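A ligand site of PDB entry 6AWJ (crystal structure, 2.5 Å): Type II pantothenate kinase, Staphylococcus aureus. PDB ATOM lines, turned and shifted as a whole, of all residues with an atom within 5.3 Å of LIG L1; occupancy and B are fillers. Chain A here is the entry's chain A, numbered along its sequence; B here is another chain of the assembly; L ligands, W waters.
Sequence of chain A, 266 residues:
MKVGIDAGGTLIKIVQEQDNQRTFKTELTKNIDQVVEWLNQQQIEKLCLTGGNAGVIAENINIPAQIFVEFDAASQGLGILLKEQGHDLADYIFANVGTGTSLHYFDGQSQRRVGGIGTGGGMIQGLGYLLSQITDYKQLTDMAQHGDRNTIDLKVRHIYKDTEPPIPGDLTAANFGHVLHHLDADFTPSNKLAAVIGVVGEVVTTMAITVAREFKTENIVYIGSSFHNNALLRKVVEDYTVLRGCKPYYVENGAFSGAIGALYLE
O of Gly 8 lies within hydrogen-bond range of OG1 of Thr 29, at 2.7 Å.
O of Lys 13 is in hydrogen-bond range of N of Asp 6, at 2.9 Å.
The side-chain hydroxyl of Ser 226 lies close to the backbone NH of Gly 121 (3.2 Å).
The backbone carbonyl oxygen (O) of Gly 98 sits at hydrogen-bond distance from the side-chain hydroxyl (OG) of Ser 226, 3.1 Å away.
The side-chain hydroxyl of Thr 29 is in hydrogen-bond range of the backbone NH of Leu 11 (3.5 Å).
OG1 of Thr 99 sits at hydrogen-bond distance from OG1 of Thr 10.
NZ of Lys 13 is in hydrogen-bond range of O of Leu 11 (3.0 Å).
The backbone carbonyl oxygen (O) of Thr 10 sits at hydrogen-bond distance from the backbone NH (N) of Thr 29.
An oxygen (O2) of LIG L1 is in hydrogen-bond range of the backbone NH of Thr 99, 3.2 Å away.
O10 of LIG L1 lies within hydrogen-bond range of O of Gly 121 (3.2 Å).
The backbone NH (N) of Gly 9 is in hydrogen-bond range of an oxygen (O1) of LIG L1 (3.5 Å).
An oxygen (O8) of LIG L1 is in hydrogen-bond range of the backbone NH (N) of Ser 226.
The backbone NH (N) of Leu 11 is in hydrogen-bond range of an oxygen (O1) of LIG L1 (2.8 Å).
An oxygen (O4) of LIG L1 is in salt-bridge range of the side-chain amino group (NZ) of Lys 13 (2.7 Å).
N of Thr 10 lies within hydrogen-bond range of O1 of LIG L1, at 3.0 Å.
O1 of LG2 L2 sits close to N of Gly 100, 3.4 Å away.
N of Ser 225 is in hydrogen-bond range of O5 of LIG L1, 3.0 Å away.
An oxygen (O4) of LIG L1 sits at hydrogen-bond distance from the side-chain hydroxyl (OG) of Ser 225, 3.0 Å away.
NE2 of Gln 125 lies within hydrogen-bond range of O9 of LIG L1, 2.9 Å away.
N of Gly 122 sits at hydrogen-bond distance from O9 of LIG L1, at 3.3 Å.
The side-chain hydroxyl of Thr 99 is in hydrogen-bond range of an oxygen (O2) of LIG L1.
Water W2 bridges OD1 of Asn 96 (2.7 Å) and O5 of LIG L1 (3.0 Å).
Water W1 lies within hydrogen-bond range of O1 of LG2 L2, O2 of LIG L1, N of Gly 100 and N of Thr 99.
The side-chain hydroxyl (OH) of Tyr 137 lies close to a nitrogen (N1) of LIG L1 (3.4 Å).
CA of Gly 8 touches O3 of LIG L1 (3.6 Å).
CD2 of Leu 28 touches N4 of LIG L1 (3.8 Å).
Val 97 touches LIG L1.
Gly 98 touches LIG L1 (CA to O6, 3.2 Å).
Gly 224 touches LIG L1.
Hydrophobic or aromatic side chains that line LIG L1: Leu 11, Leu 28 and Tyr 137.
The nearest printed residue that does not touch LIG L1 is His 228 (4.2 Å).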
ATOM      1  N   ASP A   6      -3.686  19.201  -3.185  1.00  0.00           N
ATOM      2  CA  ASP A   6      -3.890  19.199  -1.727  1.00  0.00           C
ATOM      3  C   ASP A   6      -2.935  18.164  -1.167  1.00  0.00           C
ATOM      4  O   ASP A   6      -3.186  16.955  -1.215  1.00  0.00           O
ATOM      5  CB  ASP A   6      -5.353  18.891  -1.374  1.00  0.00           C
ATOM      6  CG  ASP A   6      -5.662  19.035   0.143  1.00  0.00           C
ATOM      7  OD1 ASP A   6      -4.713  19.244   0.965  1.00  0.00           O
ATOM      8  OD2 ASP A   6      -6.884  18.924   0.510  1.00  0.00           O
ATOM      9  N   GLY A   8      -1.647  16.489   1.722  1.00  0.00           N
ATOM     10  CA  GLY A   8      -1.991  16.219   3.091  1.00  0.00           C
ATOM     11  C   GLY A   8      -0.921  15.425   3.792  1.00  0.00           C
ATOM     12  O   GLY A   8       0.180  15.187   3.258  1.00  0.00           O
ATOM     13  N   GLY A   9      -1.226  15.052   5.038  1.00  0.00           N
ATOM     14  CA  GLY A   9      -0.324  14.244   5.843  1.00  0.00           C
ATOM     15  C   GLY A   9      -0.119  12.835   5.318  1.00  0.00           C
ATOM     16  O   GLY A   9       0.965  12.273   5.438  1.00  0.00           O
ATOM     17  N   THR A  10      -1.172  12.271   4.752  1.00  0.00           N
ATOM     18  CA  THR A  10      -1.119  10.904   4.212  1.00  0.00           C
ATOM     19  C   THR A  10      -1.244  10.827   2.685  1.00  0.00           C
ATOM     20  O   THR A  10      -0.470  10.085   2.050  1.00  0.00           O
ATOM     21  CB  THR A  10      -2.218  10.006   4.807  1.00  0.00           C
ATOM     22  OG1 THR A  10      -2.375  10.308   6.198  1.00  0.00           O
ATOM     23  CG2 THR A  10      -1.854   8.561   4.629  1.00  0.00           C
ATOM     24  N   LEU A  11      -2.192  11.565   2.093  1.00  0.00           N
ATOM     25  CA  LEU A  11      -2.371  11.502   0.641  1.00  0.00           C
ATOM     26  C   LEU A  11      -2.165  12.863  -0.056  1.00  0.00           C
ATOM     27  O   LEU A  11      -2.487  13.929   0.501  1.00  0.00           O
ATOM     28  CB  LEU A  11      -3.723  10.904   0.287  1.00  0.00           C
ATOM     29  CG  LEU A  11      -4.030   9.541   0.889  1.00  0.00           C
ATOM     30  CD1 LEU A  11      -5.482   9.165   0.629  1.00  0.00           C
ATOM     31  CD2 LEU A  11      -3.119   8.433   0.362  1.00  0.00           C
ATOM     32  N   LYS A  13      -3.463  14.844  -3.205  1.00  0.00           N
ATOM     33  CA  LYS A  13      -4.577  14.864  -4.153  1.00  0.00           C
ATOM     34  C   LYS A  13      -4.303  15.864  -5.271  1.00  0.00           C
ATOM     35  O   LYS A  13      -3.981  17.012  -5.052  1.00  0.00           O
ATOM     36  CB  LYS A  13      -5.915  15.164  -3.433  1.00  0.00           C
ATOM     37  CG  LYS A  13      -6.565  13.970  -2.703  1.00  0.00           C
ATOM     38  CD  LYS A  13      -6.139  13.653  -1.253  1.00  0.00           C
ATOM     39  CE  LYS A  13      -5.404  14.755  -0.477  1.00  0.00           C
ATOM     40  NZ  LYS A  13      -5.397  14.541   0.988  1.00  0.00           N
ATOM     41  N   LEU A  28       0.595   8.807  -2.679  1.00  0.00           N
ATOM     42  CA  LEU A  28       0.986   8.800  -1.275  1.00  0.00           C
ATOM     43  C   LEU A  28       1.924   9.974  -0.940  1.00  0.00           C
ATOM     44  O   LEU A  28       2.790  10.361  -1.764  1.00  0.00           O
ATOM     45  CB  LEU A  28       1.670   7.481  -0.901  1.00  0.00           C
ATOM     46  CG  LEU A  28       0.876   6.184  -1.108  1.00  0.00           C
ATOM     47  CD1 LEU A  28       1.752   4.959  -0.808  1.00  0.00           C
ATOM     48  CD2 LEU A  28      -0.405   6.178  -0.272  1.00  0.00           C
ATOM     49  N   THR A  29       1.755  10.527   0.263  1.00  0.00           N
ATOM     50  CA  THR A  29       2.632  11.585   0.768  1.00  0.00           C
ATOM     51  C   THR A  29       4.032  11.053   0.929  1.00  0.00           C
ATOM     52  O   THR A  29       4.995  11.757   0.663  1.00  0.00           O
ATOM     53  CB  THR A  29       2.127  12.233   2.076  1.00  0.00           C
ATOM     54  OG1 THR A  29       0.952  13.006   1.794  1.00  0.00           O
ATOM     55  CG2 THR A  29       3.192  13.180   2.679  1.00  0.00           C
ATOM     56  N   ASN A  96     -14.254  17.372   7.414  1.00  0.00           N
ATOM     57  CA  ASN A  96     -13.175  16.908   6.526  1.00  0.00           C
ATOM     58  C   ASN A  96     -12.418  15.790   7.258  1.00  0.00           C
ATOM     59  O   ASN A  96     -11.649  16.048   8.155  1.00  0.00           O
ATOM     60  CB  ASN A  96     -12.235  18.058   6.148  1.00  0.00           C
ATOM     61  CG  ASN A  96     -11.322  17.700   4.987  1.00  0.00           C
ATOM     62  OD1 ASN A  96     -11.312  16.582   4.547  1.00  0.00           O
ATOM     63  ND2 ASN A  96     -10.631  18.667   4.465  1.00  0.00           N
ATOM     64  N   VAL A  97     -12.707  14.549   6.897  1.00  0.00           N
ATOM     65  CA  VAL A  97     -12.194  13.383   7.612  1.00  0.00           C
ATOM     66  C   VAL A  97     -10.970  12.803   6.920  1.00  0.00           C
ATOM     67  O   VAL A  97     -11.037  11.931   6.056  1.00  0.00           O
ATOM     68  CB  VAL A  97     -13.296  12.306   7.799  1.00  0.00           C
ATOM     69  CG1 VAL A  97     -12.782  11.164   8.666  1.00  0.00           C
ATOM     70  CG2 VAL A  97     -14.540  12.939   8.409  1.00  0.00           C
ATOM     71  N   GLY A  98      -9.829  13.322   7.325  1.00  0.00           N
ATOM     72  CA  GLY A  98      -8.543  12.952   6.722  1.00  0.00           C
ATOM     73  C   GLY A  98      -7.691  12.151   7.666  1.00  0.00           C
ATOM     74  O   GLY A  98      -8.186  11.285   8.373  1.00  0.00           O
ATOM     75  N   THR A  99      -6.410  12.458   7.696  1.00  0.00           N
ATOM     76  CA  THR A  99      -5.537  11.831   8.681  1.00  0.00           C
ATOM     77  C   THR A  99      -6.104  12.135  10.082  1.00  0.00           C
ATOM     78  O   THR A  99      -6.169  11.238  10.954  1.00  0.00           O
ATOM     79  CB  THR A  99      -4.104  12.376   8.592  1.00  0.00           C
ATOM     80  OG1 THR A  99      -3.665  12.323   7.231  1.00  0.00           O
ATOM     81  CG2 THR A  99      -3.195  11.547   9.459  1.00  0.00           C
ATOM     82  N   GLY A 100      -6.499  13.398  10.271  1.00  0.00           N
ATOM     83  CA  GLY A 100      -7.347  13.806  11.351  1.00  0.00           C
ATOM     84  C   GLY A 100      -8.598  14.435  10.782  1.00  0.00           C
ATOM     85  O   GLY A 100      -8.714  14.574   9.580  1.00  0.00           O
ATOM     86  N   GLY A 121      -8.792   9.135   9.835  1.00  0.00           N
ATOM     87  CA  GLY A 121      -8.190   8.071   9.027  1.00  0.00           C
ATOM     88  C   GLY A 121      -6.871   7.565   9.588  1.00  0.00           C
ATOM     89  O   GLY A 121      -6.559   6.388   9.486  1.00  0.00           O
ATOM     90  N   GLY A 122      -6.075   8.484  10.125  1.00  0.00           N
ATOM     91  CA  GLY A 122      -4.764   8.171  10.656  1.00  0.00           C
ATOM     92  C   GLY A 122      -4.887   7.281  11.846  1.00  0.00           C
ATOM     93  O   GLY A 122      -4.021   6.456  12.088  1.00  0.00           O
ATOM     94  N   ILE A 124      -7.443   5.145  12.122  1.00  0.00           N
ATOM     95  CA  ILE A 124      -7.887   3.861  11.598  1.00  0.00           C
ATOM     96  C   ILE A 124      -6.692   3.038  11.171  1.00  0.00           C
ATOM     97  O   ILE A 124      -6.565   1.879  11.523  1.00  0.00           O
ATOM     98  CB  ILE A 124      -8.917   4.010  10.446  1.00  0.00           C
ATOM     99  CG1 ILE A 124     -10.224   4.604  10.998  1.00  0.00           C
ATOM    100  CG2 ILE A 124      -9.172   2.650   9.745  1.00  0.00           C
ATOM    101  CD1 ILE A 124     -11.203   5.047   9.953  1.00  0.00           C
ATOM    102  N   GLN A 125      -5.780   3.675  10.471  1.00  0.00           N
ATOM    103  CA  GLN A 125      -4.504   3.014  10.047  1.00  0.00           C
ATOM    104  C   GLN A 125      -3.595   2.641  11.224  1.00  0.00           C
ATOM    105  O   GLN A 125      -3.103   1.509  11.309  1.00  0.00           O
ATOM    106  CB  GLN A 125      -3.712   3.922   9.122  1.00  0.00           C
ATOM    107  CG  GLN A 125      -4.361   4.172   7.787  1.00  0.00           C
ATOM    108  CD  GLN A 125      -3.394   4.817   6.831  1.00  0.00           C
ATOM    109  OE1 GLN A 125      -2.691   4.121   6.117  1.00  0.00           O
ATOM    110  NE2 GLN A 125      -3.274   6.150   6.880  1.00  0.00           N
ATOM    111  N   TYR A 137      -3.435  -0.530   3.514  1.00  0.00           N
ATOM    112  CA  TYR A 137      -4.719   0.145   3.750  1.00  0.00           C
ATOM    113  C   TYR A 137      -5.937  -0.610   3.189  1.00  0.00           C
ATOM    114  O   TYR A 137      -6.974  -0.736   3.842  1.00  0.00           O
ATOM    115  CB  TYR A 137      -4.678   1.581   3.195  1.00  0.00           C
ATOM    116  CG  TYR A 137      -6.019   2.280   3.272  1.00  0.00           C
ATOM    117  CD1 TYR A 137      -6.444   2.865   4.453  1.00  0.00           C
ATOM    118  CD2 TYR A 137      -6.877   2.304   2.167  1.00  0.00           C
ATOM    119  CE1 TYR A 137      -7.683   3.469   4.533  1.00  0.00           C
ATOM    120  CE2 TYR A 137      -8.122   2.897   2.254  1.00  0.00           C
ATOM    121  CZ  TYR A 137      -8.512   3.474   3.440  1.00  0.00           C
ATOM    122  OH  TYR A 137      -9.714   4.100   3.530  1.00  0.00           O
ATOM    123  N   GLY A 224     -13.349  13.677   2.664  1.00  0.00           N
ATOM    124  CA  GLY A 224     -12.012  13.184   3.001  1.00  0.00           C
ATOM    125  C   GLY A 224     -11.804  11.783   2.448  1.00  0.00           C
ATOM    126  O   GLY A 224     -12.781  11.051   2.194  1.00  0.00           O
ATOM    127  N   SER A 225     -10.561  11.381   2.248  1.00  0.00           N
ATOM    128  CA  SER A 225     -10.265  10.072   1.742  1.00  0.00           C
ATOM    129  C   SER A 225     -10.608   8.903   2.684  1.00  0.00           C
ATOM    130  O   SER A 225     -10.684   7.755   2.251  1.00  0.00           O
ATOM    131  CB  SER A 225      -8.805   9.973   1.310  1.00  0.00           C
ATOM    132  OG  SER A 225      -8.527  11.016   0.391  1.00  0.00           O
ATOM    133  N   SER A 226     -10.809   9.188   3.978  1.00  0.00           N
ATOM    134  CA  SER A 226     -11.089   8.165   4.968  1.00  0.00           C
ATOM    135  C   SER A 226     -12.274   7.306   4.594  1.00  0.00           C
ATOM    136  O   SER A 226     -12.467   6.230   5.176  1.00  0.00           O
ATOM    137  CB  SER A 226     -11.334   8.773   6.361  1.00  0.00           C
ATOM    138  OG  SER A 226     -10.142   9.290   6.923  1.00  0.00           O
ATOM    139  N   HIS A 228     -12.930   6.238   1.288  1.00  0.00           N
ATOM    140  CA  HIS A 228     -12.599   5.330   0.174  1.00  0.00           C
ATOM    141  C   HIS A 228     -12.353   3.946   0.648  1.00  0.00           C
ATOM    142  O   HIS A 228     -11.551   3.738   1.563  1.00  0.00           O
ATOM    143  CB  HIS A 228     -11.293   5.714  -0.562  1.00  0.00           C
ATOM    144  CG  HIS A 228     -11.287   7.104  -1.147  1.00  0.00           C
ATOM    145  ND1 HIS A 228     -12.395   7.931  -1.213  1.00  0.00           N
ATOM    146  CD2 HIS A 228     -10.258   7.812  -1.678  1.00  0.00           C
ATOM    147  CE1 HIS A 228     -12.048   9.081  -1.760  1.00  0.00           C
ATOM    148  NE2 HIS A 228     -10.758   9.036  -2.061  1.00  0.00           N
ATOM    149  N   ALA A 255     -13.006  14.005  -1.455  1.00  0.00           N
ATOM    150  CA  ALA A 255     -11.595  14.068  -1.050  1.00  0.00           C
ATOM    151  C   ALA A 255     -10.696  15.054  -1.847  1.00  0.00           C
ATOM    152  O   ALA A 255      -9.620  15.443  -1.369  1.00  0.00           O
ATOM    153  CB  ALA A 255     -10.977  12.670  -1.103  1.00  0.00           C
ATOM    154  N   ILE B 159       2.453  17.397  10.325  1.00  0.00           N
ATOM    155  CA  ILE B 159       1.797  17.404   9.029  1.00  0.00           C
ATOM    156  C   ILE B 159       2.178  18.629   8.266  1.00  0.00           C
ATOM    157  O   ILE B 159       2.418  18.564   7.127  1.00  0.00           O
ATOM    158  CB  ILE B 159       0.292  17.407   9.130  1.00  0.00           C
ATOM    159  CG1 ILE B 159      -0.215  16.131   9.759  1.00  0.00           C
ATOM    160  CG2 ILE B 159      -0.309  17.590   7.779  1.00  0.00           C
ATOM    161  CD1 ILE B 159      -1.704  15.995   9.676  1.00  0.00           C
HETATM  162  P1  LIG L   1      -4.912  13.986   4.433  1.00  0.00           P
HETATM  163  O1  LIG L   1      -3.840  13.161   3.733  1.00  0.00           O
HETATM  164  O2  LIG L   1      -4.696  14.383   5.870  1.00  0.00           O
HETATM  165  O3  LIG L   1      -5.413  15.194   3.679  1.00  0.00           O
HETATM  166  P2  LIG L   1      -7.139  12.404   3.417  1.00  0.00           P
HETATM  167  O4  LIG L   1      -6.450  12.277   2.093  1.00  0.00           O
HETATM  168  O5  LIG L   1      -8.461  13.120   3.508  1.00  0.00           O
HETATM  169  O6  LIG L   1      -6.215  13.069   4.586  1.00  0.00           O
HETATM  170  O7  LIG L   1      -7.439  10.963   4.107  1.00  0.00           O
HETATM  171  C1  LIG L   1      -6.385  10.008   4.303  1.00  0.00           C
HETATM  172  C2  LIG L   1      -6.940   8.794   4.999  1.00  0.00           C
HETATM  173  O8  LIG L   1      -7.740   8.163   4.036  1.00  0.00           O
HETATM  174  C3  LIG L   1      -5.945   7.766   5.506  1.00  0.00           C
HETATM  175  O9  LIG L   1      -5.525   7.993   6.864  1.00  0.00           O
HETATM  176  C4  LIG L   1      -6.733   6.481   5.352  1.00  0.00           C
HETATM  177  O10 LIG L   1      -7.605   6.167   6.426  1.00  0.00           O
HETATM  178  C5  LIG L   1      -7.634   6.752   4.169  1.00  0.00           C
HETATM  179  N1  LIG L   1      -7.106   6.254   2.883  1.00  0.00           N
HETATM  180  C6  LIG L   1      -7.865   6.185   1.767  1.00  0.00           C
HETATM  181  N2  LIG L   1      -7.117   5.708   0.780  1.00  0.00           N
HETATM  182  C7  LIG L   1      -5.902   5.462   1.242  1.00  0.00           C
HETATM  183  C8  LIG L   1      -4.653   4.958   0.691  1.00  0.00           C
HETATM  184  N3  LIG L   1      -4.644   4.616  -0.590  1.00  0.00           N
HETATM  185  N4  LIG L   1      -3.552   4.865   1.460  1.00  0.00           N
HETATM  186  C9  LIG L   1      -3.602   5.236   2.734  1.00  0.00           C
HETATM  187  N5  LIG L   1      -4.727   5.722   3.297  1.00  0.00           N
HETATM  188  C10 LIG L   1      -5.872   5.843   2.618  1.00  0.00           C
HETATM  189  C1  LG2 L   2      -4.728  18.734   8.774  1.00  0.00           C
HETATM  190  C2  LG2 L   2      -5.382  19.114  10.113  1.00  0.00           C
HETATM  191  C3  LG2 L   2      -6.089  20.458   9.830  1.00  0.00           C
HETATM  192  C4  LG2 L   2      -4.358  19.255  11.230  1.00  0.00           C
HETATM  193  C5  LG2 L   2      -6.429  18.027  10.580  1.00  0.00           C
HETATM  194  O1  LG2 L   2      -5.803  16.735  10.626  1.00  0.00           O
HETATM  195  C6  LG2 L   2      -7.108  18.396  11.938  1.00  0.00           C
HETATM  196  O2  LG2 L   2      -7.844  19.348  12.079  1.00  0.00           O
HETATM  197  N1  LG2 L   2      -6.793  17.600  12.900  1.00  0.00           N
HETATM  198  C7  LG2 L   2      -7.296  17.707  14.286  1.00  0.00           C
HETATM  199  C8  LG2 L   2      -6.637  18.882  15.050  1.00  0.00           C
HETATM  200  C9  LG2 L   2      -7.470  19.111  16.331  1.00  0.00           C
HETATM  201  O3  LG2 L   2      -8.470  19.812  16.312  1.00  0.00           O
HETATM  202  N2  LG2 L   2      -7.121  18.433  17.431  1.00  0.00           N
HETATM  203  C10 LG2 L   2      -7.924  18.520  18.650  1.00  0.00           C
HETATM  204  C11 LG2 L   2      -7.239  17.679  19.715  1.00  0.00           C
HETATM  205  C12 LG2 L   2      -6.217  18.552  20.426  1.00  0.00           C
HETATM  206  C13 LG2 L   2      -6.020  18.000  21.814  1.00  0.00           C
HETATM  207  C14 LG2 L   2      -4.900  18.785  22.463  1.00  0.00           C
HETATM  208  O4  LG2 L   2      -3.679  18.267  21.909  1.00  0.00           O
HETATM  209  C15 LG2 L   2      -2.510  18.616  22.652  1.00  0.00           C
HETATM  210  O   HOH W   1      -6.044  15.659   8.282  1.00  0.00           O
HETATM  211  O   HOH W   2      -8.737  15.850   4.686  1.00  0.00           O
